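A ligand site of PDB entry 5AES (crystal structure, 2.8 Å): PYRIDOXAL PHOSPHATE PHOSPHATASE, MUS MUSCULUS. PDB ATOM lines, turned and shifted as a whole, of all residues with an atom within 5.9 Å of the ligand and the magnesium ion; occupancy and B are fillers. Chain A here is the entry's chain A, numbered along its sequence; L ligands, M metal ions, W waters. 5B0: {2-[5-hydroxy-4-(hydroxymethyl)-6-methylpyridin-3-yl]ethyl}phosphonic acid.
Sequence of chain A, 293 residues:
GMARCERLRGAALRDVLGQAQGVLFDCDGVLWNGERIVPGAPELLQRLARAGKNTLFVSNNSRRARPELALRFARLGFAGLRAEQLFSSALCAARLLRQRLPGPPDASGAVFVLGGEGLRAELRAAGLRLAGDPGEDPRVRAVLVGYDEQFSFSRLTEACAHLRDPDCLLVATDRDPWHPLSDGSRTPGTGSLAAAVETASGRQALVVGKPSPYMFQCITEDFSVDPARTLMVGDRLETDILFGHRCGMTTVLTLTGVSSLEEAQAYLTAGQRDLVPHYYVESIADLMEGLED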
ATOM      1  N   ASP A  26     -24.911  18.562   4.705  1.00  0.00           N
ATOM      2  CA  ASP A  26     -25.832  19.593   5.135  1.00  0.00           C
ATOM      3  C   ASP A  26     -26.899  19.627   4.049  1.00  0.00           C
ATOM      4  O   ASP A  26     -26.648  19.189   2.922  1.00  0.00           O
ATOM      5  CB  ASP A  26     -25.146  20.951   5.245  1.00  0.00           C
ATOM      6  CG  ASP A  26     -26.131  22.092   5.483  1.00  0.00           C
ATOM      7  OD1 ASP A  26     -26.972  21.999   6.396  1.00  0.00           O
ATOM      8  OD2 ASP A  26     -26.092  23.086   4.719  1.00  0.00           O
ATOM      9  N   CYS A  27     -28.090  20.133   4.369  1.00  0.00           N
ATOM     10  CA  CYS A  27     -29.200  20.081   3.423  1.00  0.00           C
ATOM     11  C   CYS A  27     -29.384  21.353   2.606  1.00  0.00           C
ATOM     12  O   CYS A  27     -29.137  21.372   1.402  1.00  0.00           O
ATOM     13  CB  CYS A  27     -30.494  19.753   4.156  1.00  0.00           C
ATOM     14  SG  CYS A  27     -30.442  18.178   5.004  1.00  0.00           S
ATOM     15  N   ASP A  28     -29.832  22.419   3.267  1.00  0.00           N
ATOM     16  CA  ASP A  28     -30.081  23.673   2.574  1.00  0.00           C
ATOM     17  C   ASP A  28     -28.789  24.243   2.013  1.00  0.00           C
ATOM     18  O   ASP A  28     -27.796  24.420   2.735  1.00  0.00           O
ATOM     19  CB  ASP A  28     -30.753  24.689   3.499  1.00  0.00           C
ATOM     20  CG  ASP A  28     -32.235  24.410   3.687  1.00  0.00           C
ATOM     21  OD1 ASP A  28     -33.028  24.818   2.803  1.00  0.00           O
ATOM     22  OD2 ASP A  28     -32.613  23.786   4.713  1.00  0.00           O
ATOM     23  N   GLY A  29     -28.798  24.532   0.722  1.00  0.00           N
ATOM     24  CA  GLY A  29     -27.655  25.087   0.026  1.00  0.00           C
ATOM     25  C   GLY A  29     -26.781  24.006  -0.575  1.00  0.00           C
ATOM     26  O   GLY A  29     -25.848  24.286  -1.302  1.00  0.00           O
ATOM     27  N   VAL A  30     -27.111  22.751  -0.282  1.00  0.00           N
ATOM     28  CA  VAL A  30     -26.318  21.607  -0.736  1.00  0.00           C
ATOM     29  C   VAL A  30     -27.152  20.668  -1.594  1.00  0.00           C
ATOM     30  O   VAL A  30     -26.808  20.370  -2.732  1.00  0.00           O
ATOM     31  CB  VAL A  30     -25.762  20.838   0.468  1.00  0.00           C
ATOM     32  CG1 VAL A  30     -24.896  19.686   0.021  1.00  0.00           C
ATOM     33  CG2 VAL A  30     -24.992  21.780   1.376  1.00  0.00           C
ATOM     34  N   VAL A  58     -27.495  16.606   8.057  1.00  0.00           N
ATOM     35  CA  VAL A  58     -27.582  17.581   9.135  1.00  0.00           C
ATOM     36  C   VAL A  58     -28.212  18.871   8.648  1.00  0.00           C
ATOM     37  O   VAL A  58     -28.040  19.265   7.498  1.00  0.00           O
ATOM     38  CB  VAL A  58     -26.205  17.930   9.716  1.00  0.00           C
ATOM     39  CG1 VAL A  58     -25.625  16.748  10.489  1.00  0.00           C
ATOM     40  CG2 VAL A  58     -25.280  18.376   8.596  1.00  0.00           C
ATOM     41  N   SER A  59     -28.963  19.529   9.525  1.00  0.00           N
ATOM     42  CA  SER A  59     -29.630  20.761   9.172  1.00  0.00           C
ATOM     43  C   SER A  59     -29.860  21.571  10.423  1.00  0.00           C
ATOM     44  O   SER A  59     -30.231  21.018  11.455  1.00  0.00           O
ATOM     45  CB  SER A  59     -30.960  20.445   8.482  1.00  0.00           C
ATOM     46  OG  SER A  59     -31.589  21.637   8.056  1.00  0.00           O
ATOM     47  N   ASN A  60     -29.634  22.876  10.339  1.00  0.00           N
ATOM     48  CA  ASN A  60     -29.936  23.764  11.446  1.00  0.00           C
ATOM     49  C   ASN A  60     -31.359  24.308  11.311  1.00  0.00           C
ATOM     50  O   ASN A  60     -31.810  25.140  12.110  1.00  0.00           O
ATOM     51  CB  ASN A  60     -28.906  24.889  11.530  1.00  0.00           C
ATOM     52  CG  ASN A  60     -27.648  24.477  12.297  1.00  0.00           C
ATOM     53  OD1 ASN A  60     -27.629  23.447  12.996  1.00  0.00           O
ATOM     54  ND2 ASN A  60     -26.591  25.268  12.170  1.00  0.00           N
ATOM     55  N   ASN A  61     -32.071  23.803  10.317  1.00  0.00           N
ATOM     56  CA  ASN A  61     -33.474  24.149  10.136  1.00  0.00           C
ATOM     57  C   ASN A  61     -34.346  23.475  11.191  1.00  0.00           C
ATOM     58  O   ASN A  61     -34.406  22.244  11.290  1.00  0.00           O
ATOM     59  CB  ASN A  61     -33.928  23.761   8.734  1.00  0.00           C
ATOM     60  CG  ASN A  61     -35.238  24.415   8.347  1.00  0.00           C
ATOM     61  OD1 ASN A  61     -36.101  24.617   9.189  1.00  0.00           O
ATOM     62  ND2 ASN A  61     -35.360  24.779   7.079  1.00  0.00           N
ATOM     63  N   SER A  62     -35.006  24.294  11.993  1.00  0.00           N
ATOM     64  CA  SER A  62     -35.839  23.820  13.084  1.00  0.00           C
ATOM     65  C   SER A  62     -37.319  24.020  12.790  1.00  0.00           C
ATOM     66  O   SER A  62     -38.124  24.152  13.695  1.00  0.00           O
ATOM     67  CB  SER A  62     -35.480  24.542  14.379  1.00  0.00           C
ATOM     68  OG  SER A  62     -35.560  25.954  14.255  1.00  0.00           O
ATOM     69  N   ARG A  63     -37.656  24.023  11.507  1.00  0.00           N
ATOM     70  CA  ARG A  63     -39.033  24.271  11.105  1.00  0.00           C
ATOM     71  C   ARG A  63     -39.816  22.982  10.896  1.00  0.00           C
ATOM     72  O   ARG A  63     -41.029  22.951  11.094  1.00  0.00           O
ATOM     73  CB  ARG A  63     -39.047  25.103   9.828  1.00  0.00           C
ATOM     74  CG  ARG A  63     -38.914  26.595  10.071  1.00  0.00           C
ATOM     75  CD  ARG A  63     -39.256  27.409   8.825  1.00  0.00           C
ATOM     76  NE  ARG A  63     -40.550  27.035   8.255  1.00  0.00           N
ATOM     77  CZ  ARG A  63     -41.200  27.758   7.356  1.00  0.00           C
ATOM     78  NH1 ARG A  63     -40.697  28.901   6.910  1.00  0.00           N
ATOM     79  NH2 ARG A  63     -42.365  27.326   6.887  1.00  0.00           N
ATOM     80  N   TYR A 147     -35.919  28.981  15.466  1.00  0.00           N
ATOM     81  CA  TYR A 147     -36.404  29.897  14.448  1.00  0.00           C
ATOM     82  C   TYR A 147     -37.862  30.210  14.772  1.00  0.00           C
ATOM     83  O   TYR A 147     -38.716  29.344  14.705  1.00  0.00           O
ATOM     84  CB  TYR A 147     -36.285  29.261  13.055  1.00  0.00           C
ATOM     85  CG  TYR A 147     -36.699  30.152  11.924  1.00  0.00           C
ATOM     86  CD1 TYR A 147     -35.821  31.083  11.401  1.00  0.00           C
ATOM     87  CD2 TYR A 147     -37.968  30.066  11.377  1.00  0.00           C
ATOM     88  CE1 TYR A 147     -36.192  31.902  10.369  1.00  0.00           C
ATOM     89  CE2 TYR A 147     -38.343  30.880  10.333  1.00  0.00           C
ATOM     90  CZ  TYR A 147     -37.456  31.809   9.824  1.00  0.00           C
ATOM     91  OH  TYR A 147     -37.822  32.643   8.785  1.00  0.00           O
ATOM     92  N   ASP A 174     -29.499  26.557  17.274  1.00  0.00           N
ATOM     93  CA  ASP A 174     -28.309  26.900  16.501  1.00  0.00           C
ATOM     94  C   ASP A 174     -28.011  28.388  16.594  1.00  0.00           C
ATOM     95  O   ASP A 174     -28.816  29.144  17.153  1.00  0.00           O
ATOM     96  CB  ASP A 174     -28.554  26.538  15.042  1.00  0.00           C
ATOM     97  CG  ASP A 174     -29.635  27.375  14.409  1.00  0.00           C
ATOM     98  OD1 ASP A 174     -30.832  27.070  14.622  1.00  0.00           O
ATOM     99  OD2 ASP A 174     -29.292  28.339  13.699  1.00  0.00           O
ATOM    100  N   ASP A 176     -27.050  30.230  13.662  1.00  0.00           N
ATOM    101  CA  ASP A 176     -27.015  30.791  12.315  1.00  0.00           C
ATOM    102  C   ASP A 176     -27.660  32.171  12.355  1.00  0.00           C
ATOM    103  O   ASP A 176     -28.808  32.305  12.781  1.00  0.00           O
ATOM    104  CB  ASP A 176     -27.710  29.871  11.319  1.00  0.00           C
ATOM    105  CG  ASP A 176     -26.899  28.621  10.997  1.00  0.00           C
ATOM    106  OD1 ASP A 176     -25.835  28.408  11.610  1.00  0.00           O
ATOM    107  OD2 ASP A 176     -27.334  27.855  10.121  1.00  0.00           O
ATOM    108  N   HIS A 179     -30.497  33.747   6.925  1.00  0.00           N
ATOM    109  CA  HIS A 179     -30.571  32.799   5.817  1.00  0.00           C
ATOM    110  C   HIS A 179     -31.074  33.495   4.566  1.00  0.00           C
ATOM    111  O   HIS A 179     -31.929  34.379   4.649  1.00  0.00           O
ATOM    112  CB  HIS A 179     -31.479  31.615   6.165  1.00  0.00           C
ATOM    113  CG  HIS A 179     -31.104  30.917   7.430  1.00  0.00           C
ATOM    114  ND1 HIS A 179     -30.033  30.053   7.508  1.00  0.00           N
ATOM    115  CD2 HIS A 179     -31.632  30.968   8.677  1.00  0.00           C
ATOM    116  CE1 HIS A 179     -29.919  29.599   8.747  1.00  0.00           C
ATOM    117  NE2 HIS A 179     -30.887  30.137   9.468  1.00  0.00           N
ATOM    118  N   PRO A 180     -30.560  33.089   3.404  1.00  0.00           N
ATOM    119  CA  PRO A 180     -31.002  33.660   2.128  1.00  0.00           C
ATOM    120  C   PRO A 180     -32.337  33.063   1.702  1.00  0.00           C
ATOM    121  O   PRO A 180     -32.568  31.881   1.941  1.00  0.00           O
ATOM    122  CB  PRO A 180     -29.925  33.204   1.153  1.00  0.00           C
ATOM    123  CG  PRO A 180     -29.489  31.901   1.702  1.00  0.00           C
ATOM    124  CD  PRO A 180     -29.564  32.029   3.206  1.00  0.00           C
ATOM    125  N   LEU A 181     -33.191  33.868   1.082  1.00  0.00           N
ATOM    126  CA  LEU A 181     -34.465  33.381   0.557  1.00  0.00           C
ATOM    127  C   LEU A 181     -34.424  33.401  -0.965  1.00  0.00           C
ATOM    128  O   LEU A 181     -33.470  33.903  -1.565  1.00  0.00           O
ATOM    129  CB  LEU A 181     -35.623  34.231   1.057  1.00  0.00           C
ATOM    130  CG  LEU A 181     -35.818  34.300   2.575  1.00  0.00           C
ATOM    131  CD1 LEU A 181     -37.089  35.069   2.919  1.00  0.00           C
ATOM    132  CD2 LEU A 181     -35.858  32.905   3.191  1.00  0.00           C
ATOM    133  N   THR A 187     -33.596  36.255   5.934  1.00  0.00           N
ATOM    134  CA  THR A 187     -34.442  36.118   7.101  1.00  0.00           C
ATOM    135  C   THR A 187     -33.544  35.954   8.318  1.00  0.00           C
ATOM    136  O   THR A 187     -32.540  35.245   8.248  1.00  0.00           O
ATOM    137  CB  THR A 187     -35.394  34.903   6.978  1.00  0.00           C
ATOM    138  OG1 THR A 187     -36.266  34.856   8.128  1.00  0.00           O
ATOM    139  CG2 THR A 187     -34.614  33.608   6.878  1.00  0.00           C
ATOM    140  N   THR A 190     -31.855  31.792  14.084  1.00  0.00           N
ATOM    141  CA  THR A 190     -31.911  31.553  15.524  1.00  0.00           C
ATOM    142  C   THR A 190     -30.773  32.265  16.244  1.00  0.00           C
ATOM    143  O   THR A 190     -30.908  32.667  17.394  1.00  0.00           O
ATOM    144  CB  THR A 190     -31.819  30.052  15.821  1.00  0.00           C
ATOM    145  OG1 THR A 190     -32.756  29.349  14.998  1.00  0.00           O
ATOM    146  CG2 THR A 190     -32.101  29.783  17.300  1.00  0.00           C
ATOM    147  N   LYS A 210     -24.919  22.651  14.476  1.00  0.00           N
ATOM    148  CA  LYS A 210     -23.620  23.012  13.919  1.00  0.00           C
ATOM    149  C   LYS A 210     -23.343  24.490  14.143  1.00  0.00           C
ATOM    150  O   LYS A 210     -24.244  25.316  13.969  1.00  0.00           O
ATOM    151  CB  LYS A 210     -23.606  22.790  12.418  1.00  0.00           C
ATOM    152  CG  LYS A 210     -23.953  21.405  11.956  1.00  0.00           C
ATOM    153  CD  LYS A 210     -24.224  21.406  10.461  1.00  0.00           C
ATOM    154  CE  LYS A 210     -25.520  22.110  10.136  1.00  0.00           C
ATOM    155  NZ  LYS A 210     -25.646  22.364   8.678  1.00  0.00           N
ATOM    156  N   GLY A 234     -20.870  20.774   3.101  1.00  0.00           N
ATOM    157  CA  GLY A 234     -21.753  21.877   3.399  1.00  0.00           C
ATOM    158  C   GLY A 234     -21.488  23.104   2.552  1.00  0.00           C
ATOM    159  O   GLY A 234     -20.523  23.148   1.794  1.00  0.00           O
ATOM    160  N   ASP A 235     -22.336  24.118   2.687  1.00  0.00           N
ATOM    161  CA  ASP A 235     -22.254  25.305   1.863  1.00  0.00           C
ATOM    162  C   ASP A 235     -21.893  26.534   2.689  1.00  0.00           C
ATOM    163  O   ASP A 235     -21.770  27.641   2.146  1.00  0.00           O
ATOM    164  CB  ASP A 235     -23.601  25.547   1.183  1.00  0.00           C
ATOM    165  CG  ASP A 235     -24.675  25.966   2.157  1.00  0.00           C
ATOM    166  OD1 ASP A 235     -24.935  25.213   3.126  1.00  0.00           O
ATOM    167  OD2 ASP A 235     -25.252  27.052   1.972  1.00  0.00           O
ATOM    168  N   ARG A 236     -21.744  26.363   3.998  1.00  0.00           N
ATOM    169  CA  ARG A 236     -21.488  27.482   4.896  1.00  0.00           C
ATOM    170  C   ARG A 236     -20.230  27.263   5.735  1.00  0.00           C
ATOM    171  O   ARG A 236     -20.089  26.238   6.397  1.00  0.00           O
ATOM    172  CB  ARG A 236     -22.705  27.716   5.794  1.00  0.00           C
ATOM    173  CG  ARG A 236     -22.770  29.111   6.396  1.00  0.00           C
ATOM    174  CD  ARG A 236     -24.176  29.428   6.847  1.00  0.00           C
ATOM    175  NE  ARG A 236     -24.336  30.842   7.187  1.00  0.00           N
ATOM    176  CZ  ARG A 236     -25.506  31.444   7.369  1.00  0.00           C
ATOM    177  NH1 ARG A 236     -26.633  30.769   7.247  1.00  0.00           N
ATOM    178  NH2 ARG A 236     -25.540  32.740   7.677  1.00  0.00           N
ATOM    179  N   THR A 239     -20.411  27.498   9.807  1.00  0.00           N
ATOM    180  CA  THR A 239     -21.208  26.491  10.509  1.00  0.00           C
ATOM    181  C   THR A 239     -20.826  25.085  10.053  1.00  0.00           C
ATOM    182  O   THR A 239     -20.444  24.248  10.873  1.00  0.00           O
ATOM    183  CB  THR A 239     -22.742  26.674  10.312  1.00  0.00           C
ATOM    184  OG1 THR A 239     -23.165  26.006   9.123  1.00  0.00           O
ATOM    185  CG2 THR A 239     -23.123  28.142  10.234  1.00  0.00           C
ATOM    186  N   ASP A 240     -20.904  24.819   8.751  1.00  0.00           N
ATOM    187  CA  ASP A 240     -20.663  23.479   8.210  1.00  0.00           C
ATOM    188  C   ASP A 240     -19.191  23.066   8.264  1.00  0.00           C
ATOM    189  O   ASP A 240     -18.870  21.975   8.735  1.00  0.00           O
ATOM    190  CB  ASP A 240     -21.184  23.387   6.774  1.00  0.00           C
ATOM    191  CG  ASP A 240     -22.669  23.677   6.666  1.00  0.00           C
ATOM    192  OD1 ASP A 240     -23.427  23.188   7.516  1.00  0.00           O
ATOM    193  OD2 ASP A 240     -23.080  24.400   5.721  1.00  0.00           O
ATOM    194  N   VAL A 258     -24.642  29.518   0.514  1.00  0.00           N
ATOM    195  CA  VAL A 258     -24.283  30.804   1.106  1.00  0.00           C
ATOM    196  C   VAL A 258     -22.856  31.257   0.808  1.00  0.00           C
ATOM    197  O   VAL A 258     -22.650  32.372   0.309  1.00  0.00           O
ATOM    198  CB  VAL A 258     -24.471  30.745   2.600  1.00  0.00           C
ATOM    199  CG1 VAL A 258     -23.980  32.027   3.243  1.00  0.00           C
ATOM    200  CG2 VAL A 258     -25.944  30.495   2.933  1.00  0.00           C
HETATM  201  OAE 5B0 L   1     -29.444  22.838   6.216  1.00  0.00           O
HETATM  202  PAP 5B0 L   1     -29.016  24.257   6.679  1.00  0.00           P
HETATM  203  OAF 5B0 L   1     -28.155  24.147   7.971  1.00  0.00           O
HETATM  204  OAC 5B0 L   1     -28.219  24.920   5.595  1.00  0.00           O
HETATM  205  CAJ 5B0 L   1     -30.523  25.199   7.046  1.00  0.00           C
HETATM  206  CAI 5B0 L   1     -30.440  26.485   7.798  1.00  0.00           C
HETATM  207  CAN 5B0 L   1     -31.767  27.075   8.144  1.00  0.00           C
HETATM  208  CAH 5B0 L   1     -32.180  27.127   9.468  1.00  0.00           C
HETATM  209  NAK 5B0 L   1     -33.377  27.641   9.786  1.00  0.00           N
HETATM  210  CAL 5B0 L   1     -34.185  28.107   8.823  1.00  0.00           C
HETATM  211  CAA 5B0 L   1     -35.511  28.680   9.200  1.00  0.00           C
HETATM  212  CAM 5B0 L   1     -33.835  28.084   7.496  1.00  0.00           C
HETATM  213  OAD 5B0 L   1     -34.714  28.578   6.550  1.00  0.00           O
HETATM  214  CAO 5B0 L   1     -32.599  27.549   7.129  1.00  0.00           C
HETATM  215  C1  5B0 L   1     -32.167  27.483   5.693  1.00  0.00           C
HETATM  216  O2  5B0 L   1     -32.755  28.356   4.804  1.00  0.00           O
HETATM  217 MG    MG M   1     -26.620  25.060   4.360  1.00  0.00          MG
HETATM  218  O   HOH W   1     -25.479  25.620   5.966  1.00  0.00           O
HETATM  219  O   HOH W   2     -27.111  27.012   3.896  1.00  0.00           O
HETATM  220  O   HOH W   3     -33.386  27.179  12.901  1.00  0.00           O
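OAE of the ligand is in hydrogen-bond range of N of Asp 28 (3.0 Å).
An oxygen (OAF) of the ligand lies within hydrogen-bond range of the backbone NH of Asn 60 (3.1 Å).
The side-chain hydroxyl (OG) of Ser 59 sits at hydrogen-bond distance from an oxygen (OAE) of the ligand (3.1 Å).
The side-chain amino group (NZ) of Lys 210 lies within salt-bridge range of an oxygen (OAF) of the ligand (3.2 Å).
N of Asp 235 sits at hydrogen-bond distance from OD2 of Asp 240, at 3.1 Å.
The side-chain carboxylate of Asp 235 is in hydrogen-bond range of the backbone NH of Val 258 (2.9 Å).
The side-chain amino group (NZ) of Lys 210 is in salt-bridge range of the side-chain carboxylate (OD1) of Asp 240, 2.6 Å away.
ND1 of His 179 is in hydrogen-bond range of NH1 of Arg 236 (3.5 Å).
The backbone NH (N) of Tyr 147 sits at hydrogen-bond distance from the side-chain hydroxyl (OG) of Ser 62 (3.3 Å).
The side-chain hydroxyl of Tyr 147 sits at hydrogen-bond distance from the side-chain hydroxyl of Thr 187 (2.8 Å).
The backbone NH (N) of Arg 63 lies within hydrogen-bond range of the side-chain amide oxygen (OD1) of Asn 61 (2.9 Å).
OG1 of Thr 239 sits at hydrogen-bond distance from OD1 of Asp 240 (3.3 Å).
Merely in contact with the ligand: Cys 27 (3.5 Å), Asn 61 (3.3 Å), Arg 63 (3.97 Å), Tyr 147 (3.3 Å) and His 179 (3.2 Å).
Hydrophobic or aromatic side chains that line the ligand: Tyr 147 and His 179.
Ten residues have an atom within 4 Å of the ligand: Asp 26, Cys 27, Asp 28, Ser 59, Asn 60, Asn 61, Arg 63, Tyr 147, His 179 and Lys 210.
The nearest printed residue that does not touch the ligand is Val 58 (4.05 Å).
Residues that only touch the magnesium ion: Asp 240 (3.8 Å).
The magnesium ion is bound by an oxygen (OAC) of the ligand (2.0 Å), water W1 (2.0 Å), water W2 (2.1 Å), the side-chain carboxylate (OD2) of Asp 26 (2.1 Å), the side-chain carboxylate (OD1) of Asp 235 (2.1 Å) and the backbone carbonyl oxygen (O) of Asp 28 (2.1 Å).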
